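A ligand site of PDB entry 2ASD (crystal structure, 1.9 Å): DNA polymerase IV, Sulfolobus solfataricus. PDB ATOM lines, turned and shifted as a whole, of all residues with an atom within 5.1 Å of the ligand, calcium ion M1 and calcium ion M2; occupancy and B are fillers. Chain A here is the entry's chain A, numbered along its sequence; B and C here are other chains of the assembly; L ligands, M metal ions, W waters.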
ATOM      1  N   PHE A  13      26.722  -0.948  -3.219  1.00  0.00           N
ATOM      2  CA  PHE A  13      25.685  -1.531  -2.379  1.00  0.00           C
ATOM      3  C   PHE A  13      25.224  -0.488  -1.360  1.00  0.00           C
ATOM      4  O   PHE A  13      26.052   0.189  -0.740  1.00  0.00           O
ATOM      5  CB  PHE A  13      26.240  -2.764  -1.680  1.00  0.00           C
ATOM      6  CG  PHE A  13      25.350  -3.348  -0.620  1.00  0.00           C
ATOM      7  CD1 PHE A  13      24.245  -4.117  -0.958  1.00  0.00           C
ATOM      8  CD2 PHE A  13      25.635  -3.152   0.723  1.00  0.00           C
ATOM      9  CE1 PHE A  13      23.428  -4.675   0.026  1.00  0.00           C
ATOM     10  CE2 PHE A  13      24.827  -3.705   1.716  1.00  0.00           C
ATOM     11  CZ  PHE A  13      23.724  -4.460   1.358  1.00  0.00           C
ATOM     12  N   ASP A  15      22.643   0.180   2.005  1.00  0.00           N
ATOM     13  CA  ASP A  15      21.978  -0.455   3.128  1.00  0.00           C
ATOM     14  C   ASP A  15      21.501   0.678   4.048  1.00  0.00           C
ATOM     15  O   ASP A  15      22.334   1.396   4.597  1.00  0.00           O
ATOM     16  CB  ASP A  15      22.961  -1.386   3.845  1.00  0.00           C
ATOM     17  CG  ASP A  15      22.305  -2.249   4.907  1.00  0.00           C
ATOM     18  OD1 ASP A  15      21.337  -1.799   5.543  1.00  0.00           O
ATOM     19  OD2 ASP A  15      22.704  -3.394   5.197  1.00  0.00           O
ATOM     20  N   PHE A  16      20.198   0.847   4.197  1.00  0.00           N
ATOM     21  CA  PHE A  16      19.662   1.998   4.951  1.00  0.00           C
ATOM     22  C   PHE A  16      19.917   1.790   6.446  1.00  0.00           C
ATOM     23  O   PHE A  16      19.842   0.669   6.942  1.00  0.00           O
ATOM     24  CB  PHE A  16      18.154   2.201   4.704  1.00  0.00           C
ATOM     25  CG  PHE A  16      17.731   2.172   3.242  1.00  0.00           C
ATOM     26  CD1 PHE A  16      18.627   2.392   2.212  1.00  0.00           C
ATOM     27  CD2 PHE A  16      16.402   1.912   2.912  1.00  0.00           C
ATOM     28  CE1 PHE A  16      18.220   2.355   0.889  1.00  0.00           C
ATOM     29  CE2 PHE A  16      15.994   1.874   1.579  1.00  0.00           C
ATOM     30  CZ  PHE A  16      16.897   2.086   0.578  1.00  0.00           C
ATOM     31  N   ASP A  17      20.246   2.859   7.164  1.00  0.00           N
ATOM     32  CA  ASP A  17      20.612   2.748   8.580  1.00  0.00           C
ATOM     33  C   ASP A  17      19.387   2.600   9.475  1.00  0.00           C
ATOM     34  O   ASP A  17      18.392   3.274   9.280  1.00  0.00           O
ATOM     35  CB  ASP A  17      21.420   3.963   9.031  1.00  0.00           C
ATOM     36  CG  ASP A  17      22.715   4.148   8.271  1.00  0.00           C
ATOM     37  OD1 ASP A  17      23.406   3.143   7.967  1.00  0.00           O
ATOM     38  OD2 ASP A  17      23.138   5.279   7.929  1.00  0.00           O
ATOM     39  N   TYR A  18      19.526   1.729  10.487  1.00  0.00           N
ATOM     40  CA  TYR A  18      18.449   1.330  11.401  1.00  0.00           C
ATOM     41  C   TYR A  18      17.050   1.626  10.865  1.00  0.00           C
ATOM     42  O   TYR A  18      16.260   2.318  11.487  1.00  0.00           O
ATOM     43  CB  TYR A  18      18.669   1.919  12.798  1.00  0.00           C
ATOM     44  CG  TYR A  18      18.799   3.414  12.860  1.00  0.00           C
ATOM     45  CD1 TYR A  18      17.766   4.196  13.370  1.00  0.00           C
ATOM     46  CD2 TYR A  18      19.956   4.064  12.432  1.00  0.00           C
ATOM     47  CE1 TYR A  18      17.866   5.589  13.444  1.00  0.00           C
ATOM     48  CE2 TYR A  18      20.068   5.454  12.484  1.00  0.00           C
ATOM     49  CZ  TYR A  18      19.021   6.202  12.996  1.00  0.00           C
ATOM     50  OH  TYR A  18      19.122   7.573  13.059  1.00  0.00           O
ATOM     51  N   PHE A  19      16.738   1.026   9.725  1.00  0.00           N
ATOM     52  CA  PHE A  19      15.717   1.564   8.830  1.00  0.00           C
ATOM     53  C   PHE A  19      14.351   1.872   9.455  1.00  0.00           C
ATOM     54  O   PHE A  19      13.894   3.005   9.391  1.00  0.00           O
ATOM     55  CB  PHE A  19      15.545   0.690   7.579  1.00  0.00           C
ATOM     56  CG  PHE A  19      14.614   1.278   6.567  1.00  0.00           C
ATOM     57  CD1 PHE A  19      14.821   2.565   6.081  1.00  0.00           C
ATOM     58  CD2 PHE A  19      13.526   0.561   6.107  1.00  0.00           C
ATOM     59  CE1 PHE A  19      13.954   3.118   5.154  1.00  0.00           C
ATOM     60  CE2 PHE A  19      12.654   1.123   5.181  1.00  0.00           C
ATOM     61  CZ  PHE A  19      12.876   2.406   4.704  1.00  0.00           C
ATOM     62  N   TYR A  20      13.682   0.881  10.057  1.00  0.00           N
ATOM     63  CA  TYR A  20      12.326   1.120  10.541  1.00  0.00           C
ATOM     64  C   TYR A  20      12.293   2.204  11.618  1.00  0.00           C
ATOM     65  O   TYR A  20      11.405   3.053  11.625  1.00  0.00           O
ATOM     66  CB  TYR A  20      11.690  -0.155  11.100  1.00  0.00           C
ATOM     67  CG  TYR A  20      11.396  -1.258  10.098  1.00  0.00           C
ATOM     68  CD1 TYR A  20      11.785  -1.151   8.765  1.00  0.00           C
ATOM     69  CD2 TYR A  20      10.713  -2.401  10.500  1.00  0.00           C
ATOM     70  CE1 TYR A  20      11.504  -2.168   7.853  1.00  0.00           C
ATOM     71  CE2 TYR A  20      10.443  -3.413   9.617  1.00  0.00           C
ATOM     72  CZ  TYR A  20      10.840  -3.301   8.293  1.00  0.00           C
ATOM     73  OH  TYR A  20      10.554  -4.323   7.432  1.00  0.00           O
ATOM     74  N   VAL A  51      11.314  -7.676  18.744  1.00  0.00           N
ATOM     75  CA  VAL A  51      11.828  -6.409  18.235  1.00  0.00           C
ATOM     76  C   VAL A  51      12.163  -6.612  16.755  1.00  0.00           C
ATOM     77  O   VAL A  51      12.864  -7.561  16.400  1.00  0.00           O
ATOM     78  CB  VAL A  51      13.101  -5.969  19.011  1.00  0.00           C
ATOM     79  CG1 VAL A  51      13.697  -4.693  18.405  1.00  0.00           C
ATOM     80  CG2 VAL A  51      12.791  -5.750  20.489  1.00  0.00           C
ATOM     81  N   ALA A  52      11.632  -5.757  15.893  1.00  0.00           N
ATOM     82  CA  ALA A  52      12.021  -5.753  14.490  1.00  0.00           C
ATOM     83  C   ALA A  52      13.377  -5.064  14.358  1.00  0.00           C
ATOM     84  O   ALA A  52      14.281  -5.565  13.687  1.00  0.00           O
ATOM     85  CB  ALA A  52      10.991  -5.024  13.656  1.00  0.00           C
ATOM     86  N   THR A  53      13.511  -3.902  14.990  1.00  0.00           N
ATOM     87  CA  THR A  53      14.785  -3.205  15.105  1.00  0.00           C
ATOM     88  C   THR A  53      14.715  -2.119  16.164  1.00  0.00           C
ATOM     89  O   THR A  53      13.642  -1.750  16.627  1.00  0.00           O
ATOM     90  CB  THR A  53      15.172  -2.590  13.742  1.00  0.00           C
ATOM     91  OG1 THR A  53      16.562  -2.241  13.737  1.00  0.00           O
ATOM     92  CG2 THR A  53      14.453  -1.269  13.497  1.00  0.00           C
ATOM     93  N   ALA A  54      15.880  -1.610  16.547  1.00  0.00           N
ATOM     94  CA  ALA A  54      15.954  -0.438  17.415  1.00  0.00           C
ATOM     95  C   ALA A  54      17.010   0.531  16.895  1.00  0.00           C
ATOM     96  O   ALA A  54      17.915   0.116  16.184  1.00  0.00           O
ATOM     97  CB  ALA A  54      16.262  -0.869  18.846  1.00  0.00           C
ATOM     98  N   TYR A  56      20.266   3.160  17.332  1.00  0.00           N
ATOM     99  CA  TYR A  56      21.559   2.794  17.925  1.00  0.00           C
ATOM    100  C   TYR A  56      21.645   3.119  19.413  1.00  0.00           C
ATOM    101  O   TYR A  56      22.413   2.491  20.127  1.00  0.00           O
ATOM    102  CB  TYR A  56      22.732   3.413  17.135  1.00  0.00           C
ATOM    103  CG  TYR A  56      23.044   2.581  15.907  1.00  0.00           C
ATOM    104  CD1 TYR A  56      22.317   2.750  14.729  1.00  0.00           C
ATOM    105  CD2 TYR A  56      24.019   1.583  15.952  1.00  0.00           C
ATOM    106  CE1 TYR A  56      22.582   1.967  13.605  1.00  0.00           C
ATOM    107  CE2 TYR A  56      24.282   0.786  14.839  1.00  0.00           C
ATOM    108  CZ  TYR A  56      23.562   0.982  13.670  1.00  0.00           C
ATOM    109  OH  TYR A  56      23.814   0.202  12.557  1.00  0.00           O
ATOM    110  N   ARG A  59      20.178   0.179  20.966  1.00  0.00           N
ATOM    111  CA  ARG A  59      21.061  -0.914  20.577  1.00  0.00           C
ATOM    112  C   ARG A  59      22.365  -0.953  21.381  1.00  0.00           C
ATOM    113  O   ARG A  59      22.998  -2.002  21.493  1.00  0.00           O
ATOM    114  CB  ARG A  59      21.377  -0.786  19.089  1.00  0.00           C
ATOM    115  CG  ARG A  59      21.589  -2.095  18.370  1.00  0.00           C
ATOM    116  CD  ARG A  59      21.892  -1.905  16.903  1.00  0.00           C
ATOM    117  NE  ARG A  59      20.682  -1.634  16.143  1.00  0.00           N
ATOM    118  CZ  ARG A  59      20.595  -1.730  14.816  1.00  0.00           C
ATOM    119  NH1 ARG A  59      21.643  -2.091  14.094  1.00  0.00           N
ATOM    120  NH2 ARG A  59      19.439  -1.468  14.221  1.00  0.00           N
ATOM    121  N   ALA A  65      17.436  -6.564  17.057  1.00  0.00           N
ATOM    122  CA  ALA A  65      16.447  -7.323  16.299  1.00  0.00           C
ATOM    123  C   ALA A  65      16.354  -8.773  16.776  1.00  0.00           C
ATOM    124  O   ALA A  65      17.373  -9.401  17.059  1.00  0.00           O
ATOM    125  CB  ALA A  65      16.767  -7.275  14.811  1.00  0.00           C
ATOM    126  N   GLY A  66      15.125  -9.274  16.869  1.00  0.00           N
ATOM    127  CA  GLY A  66      14.877 -10.671  17.158  1.00  0.00           C
ATOM    128  C   GLY A  66      14.568 -11.005  18.605  1.00  0.00           C
ATOM    129  O   GLY A  66      13.978 -12.048  18.869  1.00  0.00           O
ATOM    130  N   MET A  84       5.277  -1.886  14.754  1.00  0.00           N
ATOM    131  CA  MET A  84       5.825  -1.903  13.409  1.00  0.00           C
ATOM    132  C   MET A  84       4.734  -1.488  12.439  1.00  0.00           C
ATOM    133  O   MET A  84       3.639  -2.043  12.451  1.00  0.00           O
ATOM    134  CB  MET A  84       6.321  -3.299  13.049  1.00  0.00           C
ATOM    135  CG  MET A  84       7.152  -3.307  11.762  1.00  0.00           C
ATOM    136  SD  MET A  84       7.627  -4.919  11.204  1.00  0.00           S
ATOM    137  CE  MET A  84       6.081  -5.640  10.759  1.00  0.00           C
ATOM    138  N   ILE A 112      13.899  -4.826   1.752  1.00  0.00           N
ATOM    139  CA  ILE A 112      13.229  -3.572   2.065  1.00  0.00           C
ATOM    140  C   ILE A 112      14.190  -2.389   2.223  1.00  0.00           C
ATOM    141  O   ILE A 112      13.779  -1.246   2.075  1.00  0.00           O
ATOM    142  CB  ILE A 112      12.343  -3.726   3.315  1.00  0.00           C
ATOM    143  CG1 ILE A 112      11.327  -2.572   3.393  1.00  0.00           C
ATOM    144  CG2 ILE A 112      13.188  -3.826   4.585  1.00  0.00           C
ATOM    145  CD1 ILE A 112      10.062  -2.938   4.131  1.00  0.00           C
ATOM    146  N   ASP A 113      15.466  -2.655   2.497  1.00  0.00           N
ATOM    147  CA  ASP A 113      16.427  -1.580   2.696  1.00  0.00           C
ATOM    148  C   ASP A 113      17.808  -1.783   2.050  1.00  0.00           C
ATOM    149  O   ASP A 113      18.785  -1.144   2.447  1.00  0.00           O
ATOM    150  CB  ASP A 113      16.565  -1.282   4.190  1.00  0.00           C
ATOM    151  CG  ASP A 113      17.469  -2.275   4.913  1.00  0.00           C
ATOM    152  OD1 ASP A 113      17.611  -3.453   4.500  1.00  0.00           O
ATOM    153  OD2 ASP A 113      18.062  -1.929   5.932  1.00  0.00           O
ATOM    154  N   GLU A 114      17.874  -2.649   1.041  1.00  0.00           N
ATOM    155  CA  GLU A 114      19.136  -2.913   0.344  1.00  0.00           C
ATOM    156  C   GLU A 114      18.966  -2.935  -1.148  1.00  0.00           C
ATOM    157  O   GLU A 114      17.951  -3.415  -1.663  1.00  0.00           O
ATOM    158  CB  GLU A 114      19.688  -4.273   0.722  1.00  0.00           C
ATOM    159  CG  GLU A 114      20.138  -4.403   2.152  1.00  0.00           C
ATOM    160  CD  GLU A 114      20.370  -5.858   2.514  1.00  0.00           C
ATOM    161  OE1 GLU A 114      19.512  -6.683   2.147  1.00  0.00           O
ATOM    162  OE2 GLU A 114      21.394  -6.168   3.138  1.00  0.00           O
ATOM    163  N   LYS A 160      28.775  -5.868   0.081  1.00  0.00           N
ATOM    164  CA  LYS A 160      27.996  -5.989   1.304  1.00  0.00           C
ATOM    165  C   LYS A 160      28.891  -5.948   2.529  1.00  0.00           C
ATOM    166  O   LYS A 160      28.592  -5.261   3.505  1.00  0.00           O
ATOM    167  CB  LYS A 160      27.143  -7.266   1.317  1.00  0.00           C
ATOM    168  CG  LYS A 160      26.241  -7.359   2.549  1.00  0.00           C
ATOM    169  CD  LYS A 160      25.431  -8.646   2.589  1.00  0.00           C
ATOM    170  CE  LYS A 160      23.971  -8.433   2.259  1.00  0.00           C
ATOM    171  NZ  LYS A 160      23.078  -8.856   3.369  1.00  0.00           N
ATOM    172  N   LYS A 167      29.154   0.775   8.713  1.00  0.00           N
ATOM    173  CA  LYS A 167      27.840   1.143   9.264  1.00  0.00           C
ATOM    174  C   LYS A 167      27.926   2.144  10.432  1.00  0.00           C
ATOM    175  O   LYS A 167      29.005   2.428  10.942  1.00  0.00           O
ATOM    176  CB  LYS A 167      27.018  -0.107   9.606  1.00  0.00           C
ATOM    177  CG  LYS A 167      26.147  -0.537   8.438  1.00  0.00           C
ATOM    178  CD  LYS A 167      25.274  -1.724   8.774  1.00  0.00           C
ATOM    179  CE  LYS A 167      24.629  -2.243   7.519  1.00  0.00           C
ATOM    180  NZ  LYS A 167      23.779  -3.437   7.783  1.00  0.00           N
ATOM    181  N   PRO A 168      26.784   2.537  10.970  1.00  0.00           N
ATOM    182  CA  PRO A 168      26.268   3.903  10.970  1.00  0.00           C
ATOM    183  C   PRO A 168      26.814   4.907   9.946  1.00  0.00           C
ATOM    184  O   PRO A 168      27.939   5.370  10.042  1.00  0.00           O
ATOM    185  CB  PRO A 168      26.537   4.308  12.414  1.00  0.00           C
ATOM    186  CG  PRO A 168      26.434   2.921  13.153  1.00  0.00           C
ATOM    187  CD  PRO A 168      26.172   1.818  12.079  1.00  0.00           C
ATOM    188  P    DA B  12      23.409 -15.048   7.300  1.00  0.00           P
ATOM    189  OP1  DA B  12      24.663 -14.576   6.684  1.00  0.00           O
ATOM    190  OP2  DA B  12      23.355 -15.164   8.769  1.00  0.00           O
ATOM    191  O5'  DA B  12      22.226 -14.089   6.839  1.00  0.00           O
ATOM    192  C5'  DA B  12      22.171 -13.634   5.500  1.00  0.00           C
ATOM    193  C4'  DA B  12      20.977 -12.710   5.381  1.00  0.00           C
ATOM    194  O4'  DA B  12      19.765 -13.458   5.673  1.00  0.00           O
ATOM    195  C3'  DA B  12      21.046 -11.534   6.369  1.00  0.00           C
ATOM    196  O3'  DA B  12      21.102 -10.296   5.654  1.00  0.00           O
ATOM    197  C2'  DA B  12      19.810 -11.759   7.245  1.00  0.00           C
ATOM    198  C1'  DA B  12      18.897 -12.631   6.391  1.00  0.00           C
ATOM    199  N9   DA B  12      17.942 -13.430   7.165  1.00  0.00           N
ATOM    200  C8   DA B  12      18.216 -14.289   8.186  1.00  0.00           C
ATOM    201  N7   DA B  12      17.154 -14.871   8.708  1.00  0.00           N
ATOM    202  C5   DA B  12      16.109 -14.355   7.955  1.00  0.00           C
ATOM    203  C6   DA B  12      14.711 -14.571   8.011  1.00  0.00           C
ATOM    204  N6   DA B  12      14.142 -15.406   8.886  1.00  0.00           N
ATOM    205  N1   DA B  12      13.940 -13.902   7.137  1.00  0.00           N
ATOM    206  C2   DA B  12      14.522 -13.070   6.251  1.00  0.00           C
ATOM    207  N3   DA B  12      15.830 -12.776   6.112  1.00  0.00           N
ATOM    208  C4   DA B  12      16.569 -13.467   7.008  1.00  0.00           C
ATOM    209  P   DDG B  13      21.037  -8.898   6.412  1.00  0.00           P
ATOM    210  OP1 DDG B  13      21.887  -7.929   5.667  1.00  0.00           O
ATOM    211  OP2 DDG B  13      21.251  -9.046   7.860  1.00  0.00           O
ATOM    212  O5' DDG B  13      19.496  -8.506   6.199  1.00  0.00           O
ATOM    213  C5' DDG B  13      18.951  -8.512   4.886  1.00  0.00           C
ATOM    214  C4' DDG B  13      17.470  -8.187   4.908  1.00  0.00           C
ATOM    215  O4' DDG B  13      16.740  -9.287   5.514  1.00  0.00           O
ATOM    216  C3' DDG B  13      17.092  -6.913   5.650  1.00  0.00           C
ATOM    217  C2' DDG B  13      16.048  -7.332   6.682  1.00  0.00           C
ATOM    218  C1' DDG B  13      15.681  -8.771   6.297  1.00  0.00           C
ATOM    219  N9  DDG B  13      15.523  -9.645   7.442  1.00  0.00           N
ATOM    220  C8  DDG B  13      16.533 -10.218   8.197  1.00  0.00           C
ATOM    221  N7  DDG B  13      16.090 -10.979   9.163  1.00  0.00           N
ATOM    222  C5  DDG B  13      14.707 -10.904   9.027  1.00  0.00           C
ATOM    223  C6  DDG B  13      13.684 -11.521   9.786  1.00  0.00           C
ATOM    224  O6  DDG B  13      13.825 -12.271  10.747  1.00  0.00           O
ATOM    225  N1  DDG B  13      12.403 -11.192   9.352  1.00  0.00           N
ATOM    226  C2  DDG B  13      12.158 -10.385   8.278  1.00  0.00           C
ATOM    227  N2  DDG B  13      10.867 -10.174   7.985  1.00  0.00           N
ATOM    228  N3  DDG B  13      13.107  -9.780   7.545  1.00  0.00           N
ATOM    229  C4  DDG B  13      14.347 -10.100   7.982  1.00  0.00           C
ATOM    230  P   8OG C   6       5.390 -13.968  20.051  1.00  0.00           P
ATOM    231  OP1 8OG C   6       4.249 -13.749  21.020  1.00  0.00           O
ATOM    232  OP2 8OG C   6       5.617 -15.307  19.421  1.00  0.00           O
ATOM    233  O5' 8OG C   6       5.265 -12.892  18.878  1.00  0.00           O
ATOM    234  C5' 8OG C   6       6.348 -12.727  17.983  1.00  0.00           C
ATOM    235  C4' 8OG C   6       5.980 -12.011  16.718  1.00  0.00           C
ATOM    236  O4' 8OG C   6       6.981 -11.146  16.172  1.00  0.00           O
ATOM    237  C3' 8OG C   6       5.267 -12.503  15.719  1.00  0.00           C
ATOM    238  O3' 8OG C   6       4.277 -11.854  15.383  1.00  0.00           O
ATOM    239  C2' 8OG C   6       6.261 -12.964  14.690  1.00  0.00           C
ATOM    240  C1' 8OG C   6       7.342 -11.987  15.040  1.00  0.00           C
ATOM    241  N9  8OG C   6       8.674 -12.041  14.829  1.00  0.00           N
ATOM    242  C8  8OG C   6       9.449 -12.830  15.542  1.00  0.00           C
ATOM    243  N7  8OG C   6      10.747 -12.631  15.273  1.00  0.00           N
ATOM    244  C5  8OG C   6      10.776 -11.615  14.399  1.00  0.00           C
ATOM    245  C6  8OG C   6      11.817 -10.871  13.689  1.00  0.00           C
ATOM    246  O6  8OG C   6      13.022 -11.165  13.868  1.00  0.00           O
ATOM    247  N1  8OG C   6      11.443  -9.885  12.866  1.00  0.00           N
ATOM    248  C2  8OG C   6      10.151  -9.549  12.653  1.00  0.00           C
ATOM    249  N2  8OG C   6       9.870  -8.527  11.803  1.00  0.00           N
ATOM    250  N3  8OG C   6       9.142 -10.186  13.271  1.00  0.00           N
ATOM    251  C4  8OG C   6       9.379 -11.177  14.124  1.00  0.00           C
ATOM    252  O8  8OG C   6       9.005 -13.724  16.337  1.00  0.00           O
HETATM  253  N1  LIG L   1      14.080  -6.468  10.241  1.00  0.00           N
HETATM  254  C1  LIG L   1      13.136  -7.229  10.844  1.00  0.00           C
HETATM  255  N2  LIG L   1      13.493  -8.293  11.568  1.00  0.00           N
HETATM  256  C2  LIG L   1      14.784  -8.614  11.731  1.00  0.00           C
HETATM  257  C3  LIG L   1      15.774  -7.849  11.145  1.00  0.00           C
HETATM  258  C4  LIG L   1      15.386  -6.757  10.393  1.00  0.00           C
HETATM  259  O1  LIG L   1      11.917  -6.959  10.736  1.00  0.00           O
HETATM  260  N3  LIG L   1      15.126  -9.724  12.496  1.00  0.00           N
HETATM  261  C5  LIG L   1      13.678  -5.301   9.461  1.00  0.00           C
HETATM  262  C6  LIG L   1      13.819  -4.064  10.353  1.00  0.00           C
HETATM  263  C7  LIG L   1      15.131  -3.435   9.923  1.00  0.00           C
HETATM  264  C8  LIG L   1      15.190  -3.799   8.444  1.00  0.00           C
HETATM  265  O2  LIG L   1      14.551  -5.069   8.372  1.00  0.00           O
HETATM  266  O3  LIG L   1      15.157  -2.037  10.153  1.00  0.00           O
HETATM  267  C9  LIG L   1      16.589  -3.853   7.867  1.00  0.00           C
HETATM  268  O4  LIG L   1      17.374  -4.812   8.559  1.00  0.00           O
HETATM  269  P1  LIG L   1      18.734  -4.460   9.118  1.00  0.00           P
HETATM  270  O5  LIG L   1      19.368  -5.737   9.550  1.00  0.00           O
HETATM  271  O6  LIG L   1      19.527  -3.782   8.025  1.00  0.00           O
HETATM  272  O7  LIG L   1      18.584  -3.622  10.353  1.00  0.00           O
HETATM  273  P2  LIG L   1      18.736  -2.131  10.524  1.00  0.00           P
HETATM  274  O8  LIG L   1      18.645  -1.347   9.257  1.00  0.00           O
HETATM  275  O9  LIG L   1      17.636  -1.683  11.450  1.00  0.00           O
HETATM  276  O10 LIG L   1      20.084  -1.898  11.184  1.00  0.00           O
HETATM  277  P3  LIG L   1      21.422  -1.606  10.491  1.00  0.00           P
HETATM  278  O11 LIG L   1      21.468  -1.635   8.973  1.00  0.00           O
HETATM  279  O12 LIG L   1      22.398  -2.671  10.947  1.00  0.00           O
HETATM  280  O13 LIG L   1      21.852  -0.211  10.870  1.00  0.00           O
HETATM  281 CA    CA M   1      21.824  -5.628   5.342  1.00  0.00          CA
HETATM  282 CA    CA M   2      19.874  -1.595   7.319  1.00  0.00          CA
HETATM  283  O   HOH W   1      10.239  -6.660   8.717  1.00  0.00           O
HETATM  284  O   HOH W   2      24.257  -5.890   5.609  1.00  0.00           O
HETATM  285  O   HOH W   3      19.656  -4.765   5.618  1.00  0.00           O
HETATM  286  O   HOH W   4      21.977  -5.416   7.577  1.00  0.00           O
HETATM  287  O   HOH W   5      17.989 -10.397  13.151  1.00  0.00           O
HETATM  288  O   HOH W   6      19.353  -8.597   9.669  1.00  0.00           O
HETATM  289  O   HOH W   7      25.010  -2.284  12.555  1.00  0.00           O
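N of Tyr 20 is in hydrogen-bond range of O3 of the ligand (3.3 Å).
NZ of Lys 167 is in salt-bridge range of O12 of the ligand (3.5 Å).
O6 of 8OG 6 of chain C is in hydrogen-bond range of a nitrogen (N3) of the ligand (2.9 Å).
OG1 of Thr 53 lies within hydrogen-bond range of O9 of the ligand (2.6 Å).
The backbone NH (N) of Phe 19 is in hydrogen-bond range of an oxygen (O9) of the ligand (3.3 Å).
O12 of the ligand is in salt-bridge range of NH1 of Arg 59.
An oxygen (O13) of the ligand lies within hydrogen-bond range of the side-chain hydroxyl of Tyr 56, 2.6 Å away.
O6 of DDG 13 of chain B lies within hydrogen-bond range of N3 of the ligand (3.4 Å).
O13 of the ligand lies within hydrogen-bond range of N of Tyr 18 (3.1 Å).
OD2 of Asp 15 lies close to NZ of Lys 167, 2.8 Å away.
OP1 of DDG 13 of chain B lies close to NZ of Lys 160 (2.7 Å).
OG1 of Thr 53 sits at hydrogen-bond distance from NH2 of Arg 59.
NZ of Lys 160 lies within hydrogen-bond range of O3' of DA 12 of chain B, 3.3 Å away.
The side-chain carboxylate of Glu 114 sits close to the side-chain amino group of Lys 160, at 3.2 Å.
NH2 of Arg 59 sits at hydrogen-bond distance from O of Ala 54 (2.9 Å).
Merely in contact with the ligand: Asp 17 (3.9 Å), Ala 52 (3.5 Å) and Ala 65 (3.7 Å).
Hydrophobic or aromatic side chains within 4 Å of the ligand: Tyr 18, Phe 19, Tyr 20, Ala 52, Tyr 56 and Ala 65.
Along chain A the residues within 4 Å of the ligand span positions 15 to 167.
Residues that only touch calcium ion M1: Lys 167 (3.8 Å) and Lys 160 (3.99 Å).
Within 4 Å of calcium ion M1: Asp 15, Glu 114, Lys 160, Lys 167 and DDG 13 of chain B.
Three residues have an atom within 4 Å of calcium ion M2: Asp 15, Phe 16 and Asp 113.
Water W4 is bound to calcium ion M1 (2.3 Å).
OE2 of Glu 114 is bound to calcium ion M1 (2.3 Å).
OP1 of DDG 13 of chain B is bound to calcium ion M1 (2.3 Å).
Water W3 is bound to calcium ion M1 (2.3 Å).
The side-chain carboxylate (OD2) of Asp 15 binds calcium ion M1, at 2.4 Å.
Water W2 is bound to calcium ion M1, at 2.5 Å.
Calcium ion M2 is bound by the backbone carbonyl oxygen (O) of Phe 16 (2.3 Å), an oxygen (O11) of the ligand (2.3 Å), the side-chain carboxylate (OD2) of Asp 113 (2.3 Å), an oxygen (O8) of the ligand (2.3 Å), the side-chain carboxylate (OD1) of Asp 15 (2.3 Å) and an oxygen (O6) of the ligand (2.3 Å).
Water W4 bridges NZ of Lys 167 (2.7 Å) and O5 of the ligand (3.3 Å).
Water W1 bridges O1 of the ligand (2.6 Å) and OH of Tyr 20 (2.7 Å).
Water W6 lies within hydrogen-bond range of OP2 of DDG 13 of chain B (2.7 Å) and O5 of the ligand (2.9 Å).
Water W7 bridges the side-chain hydroxyl of Tyr 56 and an oxygen (O12) of the ligand.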
